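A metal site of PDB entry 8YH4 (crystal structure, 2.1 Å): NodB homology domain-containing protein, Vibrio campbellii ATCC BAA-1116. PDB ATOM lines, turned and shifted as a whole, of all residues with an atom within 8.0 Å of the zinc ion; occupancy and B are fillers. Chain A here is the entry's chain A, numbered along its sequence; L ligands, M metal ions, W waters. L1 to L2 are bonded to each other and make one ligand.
The backbone carbonyl oxygen of His 71 sits at hydrogen-bond distance from the side-chain amide nitrogen of Asn 39 (2.8 Å).
The backbone carbonyl oxygen (O) of Tyr 37 lies within hydrogen-bond range of the backbone NH (N) of Asp 14, 3.1 Å away.
The backbone carbonyl oxygen (O) of His 75 sits at hydrogen-bond distance from the side-chain hydroxyl (OH) of Tyr 143 (3.1 Å).
A ring nitrogen (ND1) of His 71 is in hydrogen-bond range of the backbone carbonyl oxygen (O) of Arg 140, at 2.7 Å.
The side-chain hydroxyl of Ser 72 lies within hydrogen-bond range of the backbone NH of His 75, at 3.2 Å.
The backbone NH (N) of Asp 13 is in hydrogen-bond range of the backbone carbonyl oxygen (O) of Thr 268, 2.9 Å away.
The guanidinium group (NH1) of Arg 140 lies within salt-bridge range of the side-chain carboxylate (OD1) of Asp 13 (2.9 Å).
Water W2 lies within hydrogen-bond range of N1 of LIG L1 (2.5 Å), OD2 of Asp 13 (2.6 Å) and NE2 of His 269 (3.1 Å).
Water W1 bridges N1 of LIG L1 (2.7 Å) and N of Tyr 143 (2.8 Å).
The zinc ion is bound by NE2 of His 75, at 2.0 Å.
Water W2 binds the zinc ion, at 2.0 Å.
The side-chain carboxylate (OD1) of Asp 14 binds the zinc ion, at 2.2 Å.
The zinc ion is bound by a ring nitrogen (NE2) of His 71 (2.3 Å).
The zinc ion is bound by water W1, at 2.3 Å.
The zinc ion has five donor atoms within binding distance.
NE2 of His 269 lies within hydrogen-bond range of N1 of LIG L1, at 3.2 Å.
A ring nitrogen (NE2) of His 75 lies close to an oxygen (O2) of LIG L1 (3.3 Å).
An oxygen (O2) of LIG L1 is in hydrogen-bond range of the side-chain carboxylate of Asp 14.
Asp 13 touches the zinc ion.
The nearest printed residue that does not touch the zinc ion is His 269 (4.3 Å).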
ATOM      1  N   PHE A  12     -11.358  12.248 -13.879  1.00  0.00           N
ATOM      2  CA  PHE A  12     -10.400  12.237 -12.789  1.00  0.00           C
ATOM      3  C   PHE A  12     -10.462  13.560 -12.046  1.00  0.00           C
ATOM      4  O   PHE A  12     -10.383  14.625 -12.668  1.00  0.00           O
ATOM      5  CB  PHE A  12      -8.987  11.965 -13.313  1.00  0.00           C
ATOM      6  CG  PHE A  12      -8.815  10.620 -13.969  1.00  0.00           C
ATOM      7  CD1 PHE A  12      -9.247  10.414 -15.277  1.00  0.00           C
ATOM      8  CD2 PHE A  12      -8.243   9.567 -13.275  1.00  0.00           C
ATOM      9  CE1 PHE A  12      -9.097   9.177 -15.884  1.00  0.00           C
ATOM     10  CE2 PHE A  12      -8.090   8.330 -13.873  1.00  0.00           C
ATOM     11  CZ  PHE A  12      -8.523   8.135 -15.180  1.00  0.00           C
ATOM     12  N   ASP A  13     -10.595  13.499 -10.730  1.00  0.00           N
ATOM     13  CA  ASP A  13     -10.762  14.682  -9.900  1.00  0.00           C
ATOM     14  C   ASP A  13      -9.523  14.937  -9.053  1.00  0.00           C
ATOM     15  O   ASP A  13      -8.774  14.012  -8.708  1.00  0.00           O
ATOM     16  CB  ASP A  13     -11.974  14.546  -8.972  1.00  0.00           C
ATOM     17  CG  ASP A  13     -13.289  14.786  -9.684  1.00  0.00           C
ATOM     18  OD1 ASP A  13     -13.296  14.765 -10.935  1.00  0.00           O
ATOM     19  OD2 ASP A  13     -14.308  14.998  -8.989  1.00  0.00           O
ATOM     20  N   ASP A  14      -9.314  16.216  -8.734  1.00  0.00           N
ATOM     21  CA  ASP A  14      -8.388  16.745  -7.719  1.00  0.00           C
ATOM     22  C   ASP A  14      -6.941  16.856  -8.180  1.00  0.00           C
ATOM     23  O   ASP A  14      -6.054  17.142  -7.348  1.00  0.00           O
ATOM     24  CB  ASP A  14      -8.422  15.929  -6.423  1.00  0.00           C
ATOM     25  CG  ASP A  14      -9.802  15.942  -5.788  1.00  0.00           C
ATOM     26  OD1 ASP A  14     -10.772  16.310  -6.496  1.00  0.00           O
ATOM     27  OD2 ASP A  14      -9.904  15.593  -4.595  1.00  0.00           O
ATOM     28  N   GLY A  15      -6.651  16.679  -9.475  1.00  0.00           N
ATOM     29  CA  GLY A  15      -5.351  17.010  -9.992  1.00  0.00           C
ATOM     30  C   GLY A  15      -5.222  18.517 -10.162  1.00  0.00           C
ATOM     31  O   GLY A  15      -6.107  19.274  -9.755  1.00  0.00           O
ATOM     32  N   TYR A  37     -10.809  17.148 -13.806  1.00  0.00           N
ATOM     33  CA  TYR A  37     -11.362  18.271 -13.042  1.00  0.00           C
ATOM     34  C   TYR A  37     -10.287  18.742 -12.072  1.00  0.00           C
ATOM     35  O   TYR A  37     -10.058  18.110 -11.031  1.00  0.00           O
ATOM     36  CB  TYR A  37     -12.651  17.869 -12.346  1.00  0.00           C
ATOM     37  CG  TYR A  37     -13.799  17.633 -13.315  1.00  0.00           C
ATOM     38  CD1 TYR A  37     -14.635  18.682 -13.693  1.00  0.00           C
ATOM     39  CD2 TYR A  37     -14.048  16.383 -13.844  1.00  0.00           C
ATOM     40  CE1 TYR A  37     -15.679  18.494 -14.575  1.00  0.00           C
ATOM     41  CE2 TYR A  37     -15.084  16.176 -14.738  1.00  0.00           C
ATOM     42  CZ  TYR A  37     -15.901  17.236 -15.092  1.00  0.00           C
ATOM     43  OH  TYR A  37     -16.950  17.047 -15.961  1.00  0.00           O
ATOM     44  N   ASN A  39      -7.838  21.320  -9.642  1.00  0.00           N
ATOM     45  CA  ASN A  39      -7.759  22.372  -8.647  1.00  0.00           C
ATOM     46  C   ASN A  39      -6.390  23.016  -8.747  1.00  0.00           C
ATOM     47  O   ASN A  39      -5.373  22.344  -8.543  1.00  0.00           O
ATOM     48  CB  ASN A  39      -7.971  21.821  -7.225  1.00  0.00           C
ATOM     49  CG  ASN A  39      -9.211  20.967  -7.116  1.00  0.00           C
ATOM     50  OD1 ASN A  39      -9.130  19.767  -6.862  1.00  0.00           O
ATOM     51  ND2 ASN A  39     -10.381  21.585  -7.282  1.00  0.00           N
ATOM     52  N   HIS A  71     -12.660  22.445 -11.281  1.00  0.00           N
ATOM     53  CA  HIS A  71     -13.055  21.831 -10.012  1.00  0.00           C
ATOM     54  C   HIS A  71     -12.900  22.797  -8.841  1.00  0.00           C
ATOM     55  O   HIS A  71     -12.991  22.359  -7.693  1.00  0.00           O
ATOM     56  CB  HIS A  71     -12.235  20.562  -9.783  1.00  0.00           C
ATOM     57  CG  HIS A  71     -12.879  19.579  -8.849  1.00  0.00           C
ATOM     58  ND1 HIS A  71     -14.243  19.417  -8.773  1.00  0.00           N
ATOM     59  CD2 HIS A  71     -12.351  18.691  -7.981  1.00  0.00           C
ATOM     60  CE1 HIS A  71     -14.534  18.483  -7.890  1.00  0.00           C
ATOM     61  NE2 HIS A  71     -13.400  18.019  -7.392  1.00  0.00           N
ATOM     62  N   SER A  72     -12.675  24.092  -9.117  1.00  0.00           N
ATOM     63  CA  SER A  72     -12.455  25.186  -8.167  1.00  0.00           C
ATOM     64  C   SER A  72     -11.008  25.250  -7.716  1.00  0.00           C
ATOM     65  O   SER A  72     -10.280  24.257  -7.800  1.00  0.00           O
ATOM     66  CB  SER A  72     -13.387  25.090  -6.951  1.00  0.00           C
ATOM     67  OG  SER A  72     -12.903  24.149  -6.011  1.00  0.00           O
ATOM     68  N   HIS A  75     -10.681  23.369  -3.845  1.00  0.00           N
ATOM     69  CA  HIS A  75     -11.561  22.271  -3.440  1.00  0.00           C
ATOM     70  C   HIS A  75     -12.383  22.636  -2.201  1.00  0.00           C
ATOM     71  O   HIS A  75     -12.705  21.770  -1.383  1.00  0.00           O
ATOM     72  CB  HIS A  75     -10.743  20.991  -3.188  1.00  0.00           C
ATOM     73  CG  HIS A  75     -11.491  19.729  -3.483  1.00  0.00           C
ATOM     74  ND1 HIS A  75     -12.325  19.122  -2.571  1.00  0.00           N
ATOM     75  CD2 HIS A  75     -11.504  18.934  -4.584  1.00  0.00           C
ATOM     76  CE1 HIS A  75     -12.830  18.021  -3.091  1.00  0.00           C
ATOM     77  NE2 HIS A  75     -12.344  17.890  -4.313  1.00  0.00           N
ATOM     78  N   ARG A 140     -17.306  20.768 -11.990  1.00  0.00           N
ATOM     79  CA  ARG A 140     -17.853  19.763 -11.093  1.00  0.00           C
ATOM     80  C   ARG A 140     -17.636  20.251  -9.667  1.00  0.00           C
ATOM     81  O   ARG A 140     -16.528  20.680  -9.319  1.00  0.00           O
ATOM     82  CB  ARG A 140     -17.204  18.393 -11.300  1.00  0.00           C
ATOM     83  CG  ARG A 140     -17.581  17.361 -10.242  1.00  0.00           C
ATOM     84  CD  ARG A 140     -16.931  16.021 -10.525  1.00  0.00           C
ATOM     85  NE  ARG A 140     -17.600  15.273 -11.590  1.00  0.00           N
ATOM     86  CZ  ARG A 140     -17.063  14.248 -12.233  1.00  0.00           C
ATOM     87  NH1 ARG A 140     -15.835  13.854 -11.922  1.00  0.00           N
ATOM     88  NH2 ARG A 140     -17.743  13.619 -13.189  1.00  0.00           N
ATOM     89  N   LEU A 141     -18.690  20.219  -8.866  1.00  0.00           N
ATOM     90  CA  LEU A 141     -18.594  20.728  -7.501  1.00  0.00           C
ATOM     91  C   LEU A 141     -17.860  19.727  -6.623  1.00  0.00           C
ATOM     92  O   LEU A 141     -18.155  18.529  -6.676  1.00  0.00           O
ATOM     93  CB  LEU A 141     -19.971  21.012  -6.937  1.00  0.00           C
ATOM     94  CG  LEU A 141     -20.404  22.483  -6.987  1.00  0.00           C
ATOM     95  CD1 LEU A 141     -20.590  22.951  -8.427  1.00  0.00           C
ATOM     96  CD2 LEU A 141     -21.668  22.694  -6.176  1.00  0.00           C
ATOM     97  N   PRO A 142     -16.882  20.161  -5.830  1.00  0.00           N
ATOM     98  CA  PRO A 142     -16.281  19.269  -4.829  1.00  0.00           C
ATOM     99  C   PRO A 142     -17.338  18.594  -3.980  1.00  0.00           C
ATOM    100  O   PRO A 142     -18.306  19.224  -3.538  1.00  0.00           O
ATOM    101  CB  PRO A 142     -15.401  20.217  -4.010  1.00  0.00           C
ATOM    102  CG  PRO A 142     -15.009  21.290  -4.988  1.00  0.00           C
ATOM    103  CD  PRO A 142     -16.179  21.454  -5.926  1.00  0.00           C
ATOM    104  N   TYR A 143     -17.151  17.293  -3.754  1.00  0.00           N
ATOM    105  CA  TYR A 143     -17.928  16.440  -2.858  1.00  0.00           C
ATOM    106  C   TYR A 143     -19.353  16.177  -3.324  1.00  0.00           C
ATOM    107  O   TYR A 143     -20.071  15.431  -2.646  1.00  0.00           O
ATOM    108  CB  TYR A 143     -18.005  17.004  -1.428  1.00  0.00           C
ATOM    109  CG  TYR A 143     -16.727  17.646  -0.926  1.00  0.00           C
ATOM    110  CD1 TYR A 143     -15.628  16.860  -0.589  1.00  0.00           C
ATOM    111  CD2 TYR A 143     -16.632  19.017  -0.769  1.00  0.00           C
ATOM    112  CE1 TYR A 143     -14.466  17.433  -0.126  1.00  0.00           C
ATOM    113  CE2 TYR A 143     -15.461  19.601  -0.309  1.00  0.00           C
ATOM    114  CZ  TYR A 143     -14.378  18.803   0.012  1.00  0.00           C
ATOM    115  OH  TYR A 143     -13.221  19.385   0.465  1.00  0.00           O
ATOM    116  N   THR A 144     -19.789  16.743  -4.444  1.00  0.00           N
ATOM    117  CA  THR A 144     -21.211  16.880  -4.728  1.00  0.00           C
ATOM    118  C   THR A 144     -21.552  16.271  -6.083  1.00  0.00           C
ATOM    119  O   THR A 144     -21.063  16.721  -7.116  1.00  0.00           O
ATOM    120  CB  THR A 144     -21.631  18.351  -4.687  1.00  0.00           C
ATOM    121  OG1 THR A 144     -21.218  18.916  -3.433  1.00  0.00           O
ATOM    122  CG2 THR A 144     -23.135  18.490  -4.821  1.00  0.00           C
ATOM    123  N   TRP A 203     -21.644  11.973 -11.453  1.00  0.00           N
ATOM    124  CA  TRP A 203     -21.104  10.675 -11.844  1.00  0.00           C
ATOM    125  C   TRP A 203     -22.121   9.577 -11.601  1.00  0.00           C
ATOM    126  O   TRP A 203     -23.029   9.707 -10.774  1.00  0.00           O
ATOM    127  CB  TRP A 203     -19.794  10.365 -11.107  1.00  0.00           C
ATOM    128  CG  TRP A 203     -19.904  10.354  -9.608  1.00  0.00           C
ATOM    129  CD1 TRP A 203     -20.143   9.274  -8.817  1.00  0.00           C
ATOM    130  CD2 TRP A 203     -19.770  11.481  -8.732  1.00  0.00           C
ATOM    131  NE1 TRP A 203     -20.162   9.654  -7.501  1.00  0.00           N
ATOM    132  CE2 TRP A 203     -19.942  11.005  -7.413  1.00  0.00           C
ATOM    133  CE3 TRP A 203     -19.532  12.847  -8.930  1.00  0.00           C
ATOM    134  CZ2 TRP A 203     -19.874  11.835  -6.301  1.00  0.00           C
ATOM    135  CZ3 TRP A 203     -19.455  13.677  -7.822  1.00  0.00           C
ATOM    136  CH2 TRP A 203     -19.631  13.171  -6.522  1.00  0.00           C
ATOM    137  N   TRP A 212     -15.245   7.257   2.121  1.00  0.00           N
ATOM    138  CA  TRP A 212     -14.102   7.958   2.674  1.00  0.00           C
ATOM    139  C   TRP A 212     -14.130   7.843   4.198  1.00  0.00           C
ATOM    140  O   TRP A 212     -15.195   7.892   4.819  1.00  0.00           O
ATOM    141  CB  TRP A 212     -14.099   9.417   2.221  1.00  0.00           C
ATOM    142  CG  TRP A 212     -14.066   9.482   0.729  1.00  0.00           C
ATOM    143  CD1 TRP A 212     -15.134   9.602  -0.118  1.00  0.00           C
ATOM    144  CD2 TRP A 212     -12.900   9.403  -0.112  1.00  0.00           C
ATOM    145  NE1 TRP A 212     -14.713   9.607  -1.425  1.00  0.00           N
ATOM    146  CE2 TRP A 212     -13.348   9.488  -1.452  1.00  0.00           C
ATOM    147  CE3 TRP A 212     -11.535   9.271   0.139  1.00  0.00           C
ATOM    148  CZ2 TRP A 212     -12.469   9.447  -2.527  1.00  0.00           C
ATOM    149  CZ3 TRP A 212     -10.665   9.230  -0.932  1.00  0.00           C
ATOM    150  CH2 TRP A 212     -11.129   9.324  -2.256  1.00  0.00           C
ATOM    151  N   LEU A 267     -16.246   8.373 -11.960  1.00  0.00           N
ATOM    152  CA  LEU A 267     -15.418   9.257 -11.151  1.00  0.00           C
ATOM    153  C   LEU A 267     -14.303   8.449 -10.499  1.00  0.00           C
ATOM    154  O   LEU A 267     -14.531   7.353  -9.990  1.00  0.00           O
ATOM    155  CB  LEU A 267     -16.238   9.964 -10.082  1.00  0.00           C
ATOM    156  CG  LEU A 267     -15.447  10.500  -8.887  1.00  0.00           C
ATOM    157  CD1 LEU A 267     -14.598  11.696  -9.294  1.00  0.00           C
ATOM    158  CD2 LEU A 267     -16.362  10.868  -7.721  1.00  0.00           C
ATOM    159  N   THR A 268     -13.092   8.999 -10.526  1.00  0.00           N
ATOM    160  CA  THR A 268     -11.989   8.491  -9.726  1.00  0.00           C
ATOM    161  C   THR A 268     -11.006   9.633  -9.519  1.00  0.00           C
ATOM    162  O   THR A 268     -11.189  10.736 -10.031  1.00  0.00           O
ATOM    163  CB  THR A 268     -11.339   7.255 -10.375  1.00  0.00           C
ATOM    164  OG1 THR A 268     -10.434   6.649  -9.444  1.00  0.00           O
ATOM    165  CG2 THR A 268     -10.585   7.647 -11.626  1.00  0.00           C
ATOM    166  N   HIS A 269      -9.952   9.371  -8.738  1.00  0.00           N
ATOM    167  CA  HIS A 269      -8.985  10.380  -8.350  1.00  0.00           C
ATOM    168  C   HIS A 269      -7.581   9.865  -8.640  1.00  0.00           C
ATOM    169  O   HIS A 269      -7.279   8.713  -8.333  1.00  0.00           O
ATOM    170  CB  HIS A 269      -9.114  10.749  -6.874  1.00  0.00           C
ATOM    171  CG  HIS A 269     -10.488  11.186  -6.465  1.00  0.00           C
ATOM    172  ND1 HIS A 269     -11.528  10.307  -6.260  1.00  0.00           N
ATOM    173  CD2 HIS A 269     -10.994  12.417  -6.224  1.00  0.00           C
ATOM    174  CE1 HIS A 269     -12.609  10.978  -5.905  1.00  0.00           C
ATOM    175  NE2 HIS A 269     -12.313  12.266  -5.887  1.00  0.00           N
ATOM    176  N   PHE A 271      -4.907  10.572  -7.153  1.00  0.00           N
ATOM    177  CA  PHE A 271      -4.121  10.275  -5.958  1.00  0.00           C
ATOM    178  C   PHE A 271      -4.319   8.840  -5.474  1.00  0.00           C
ATOM    179  O   PHE A 271      -3.555   8.394  -4.621  1.00  0.00           O
ATOM    180  CB  PHE A 271      -4.407  11.276  -4.833  1.00  0.00           C
ATOM    181  CG  PHE A 271      -5.843  11.316  -4.338  1.00  0.00           C
ATOM    182  CD1 PHE A 271      -6.420  10.220  -3.705  1.00  0.00           C
ATOM    183  CD2 PHE A 271      -6.590  12.480  -4.432  1.00  0.00           C
ATOM    184  CE1 PHE A 271      -7.719  10.271  -3.241  1.00  0.00           C
ATOM    185  CE2 PHE A 271      -7.885  12.531  -3.958  1.00  0.00           C
ATOM    186  CZ  PHE A 271      -8.454  11.427  -3.361  1.00  0.00           C
HETATM  187  C1  LIG L   1     -15.239  12.941  -2.115  1.00  0.00           C
HETATM  188  C2  LIG L   1     -14.465  13.894  -3.023  1.00  0.00           C
HETATM  189  C3  LIG L   1     -12.958  13.704  -2.835  1.00  0.00           C
HETATM  190  C4  LIG L   1     -12.583  13.803  -1.364  1.00  0.00           C
HETATM  191  C5  LIG L   1     -13.452  12.853  -0.537  1.00  0.00           C
HETATM  192  C6  LIG L   1     -13.220  12.960   0.956  1.00  0.00           C
HETATM  193  N1  LIG L   1     -14.834  13.685  -4.419  1.00  0.00           N
HETATM  194  O1  LIG L   1     -16.601  13.172  -2.252  1.00  0.00           O
HETATM  195  O2  LIG L   1     -12.266  14.700  -3.584  1.00  0.00           O
HETATM  196  O3  LIG L   1     -11.220  13.431  -1.202  1.00  0.00           O
HETATM  197  O4  LIG L   1     -14.833  13.144  -0.765  1.00  0.00           O
HETATM  198  O5  LIG L   1     -13.226  14.321   1.377  1.00  0.00           O
HETATM  199  C1  LG2 L   2     -10.435  14.484  -0.606  1.00  0.00           C
HETATM  200  C2  LG2 L   2      -9.166  13.830  -0.049  1.00  0.00           C
HETATM  201  C3  LG2 L   2      -8.226  14.885   0.531  1.00  0.00           C
HETATM  202  C4  LG2 L   2      -7.951  15.970  -0.500  1.00  0.00           C
HETATM  203  C5  LG2 L   2      -9.266  16.559  -0.995  1.00  0.00           C
HETATM  204  C6  LG2 L   2      -9.091  17.595  -2.071  1.00  0.00           C
HETATM  205  N1  LG2 L   2      -9.493  12.822   0.946  1.00  0.00           N
HETATM  206  O1  LG2 L   2      -7.002  14.269   0.922  1.00  0.00           O
HETATM  207  O2  LG2 L   2      -7.151  16.993   0.070  1.00  0.00           O
HETATM  208  O3  LG2 L   2     -10.078  15.504  -1.548  1.00  0.00           O
HETATM  209  O4  LG2 L   2      -8.082  17.213  -2.995  1.00  0.00           O
HETATM  210 ZN    ZN M   1     -12.816  16.569  -5.773  1.00  0.00          ZN
HETATM  211  O   HOH W   1     -14.936  16.280  -5.061  1.00  0.00           O
HETATM  212  O   HOH W   2     -13.823  14.907  -6.409  1.00  0.00           O
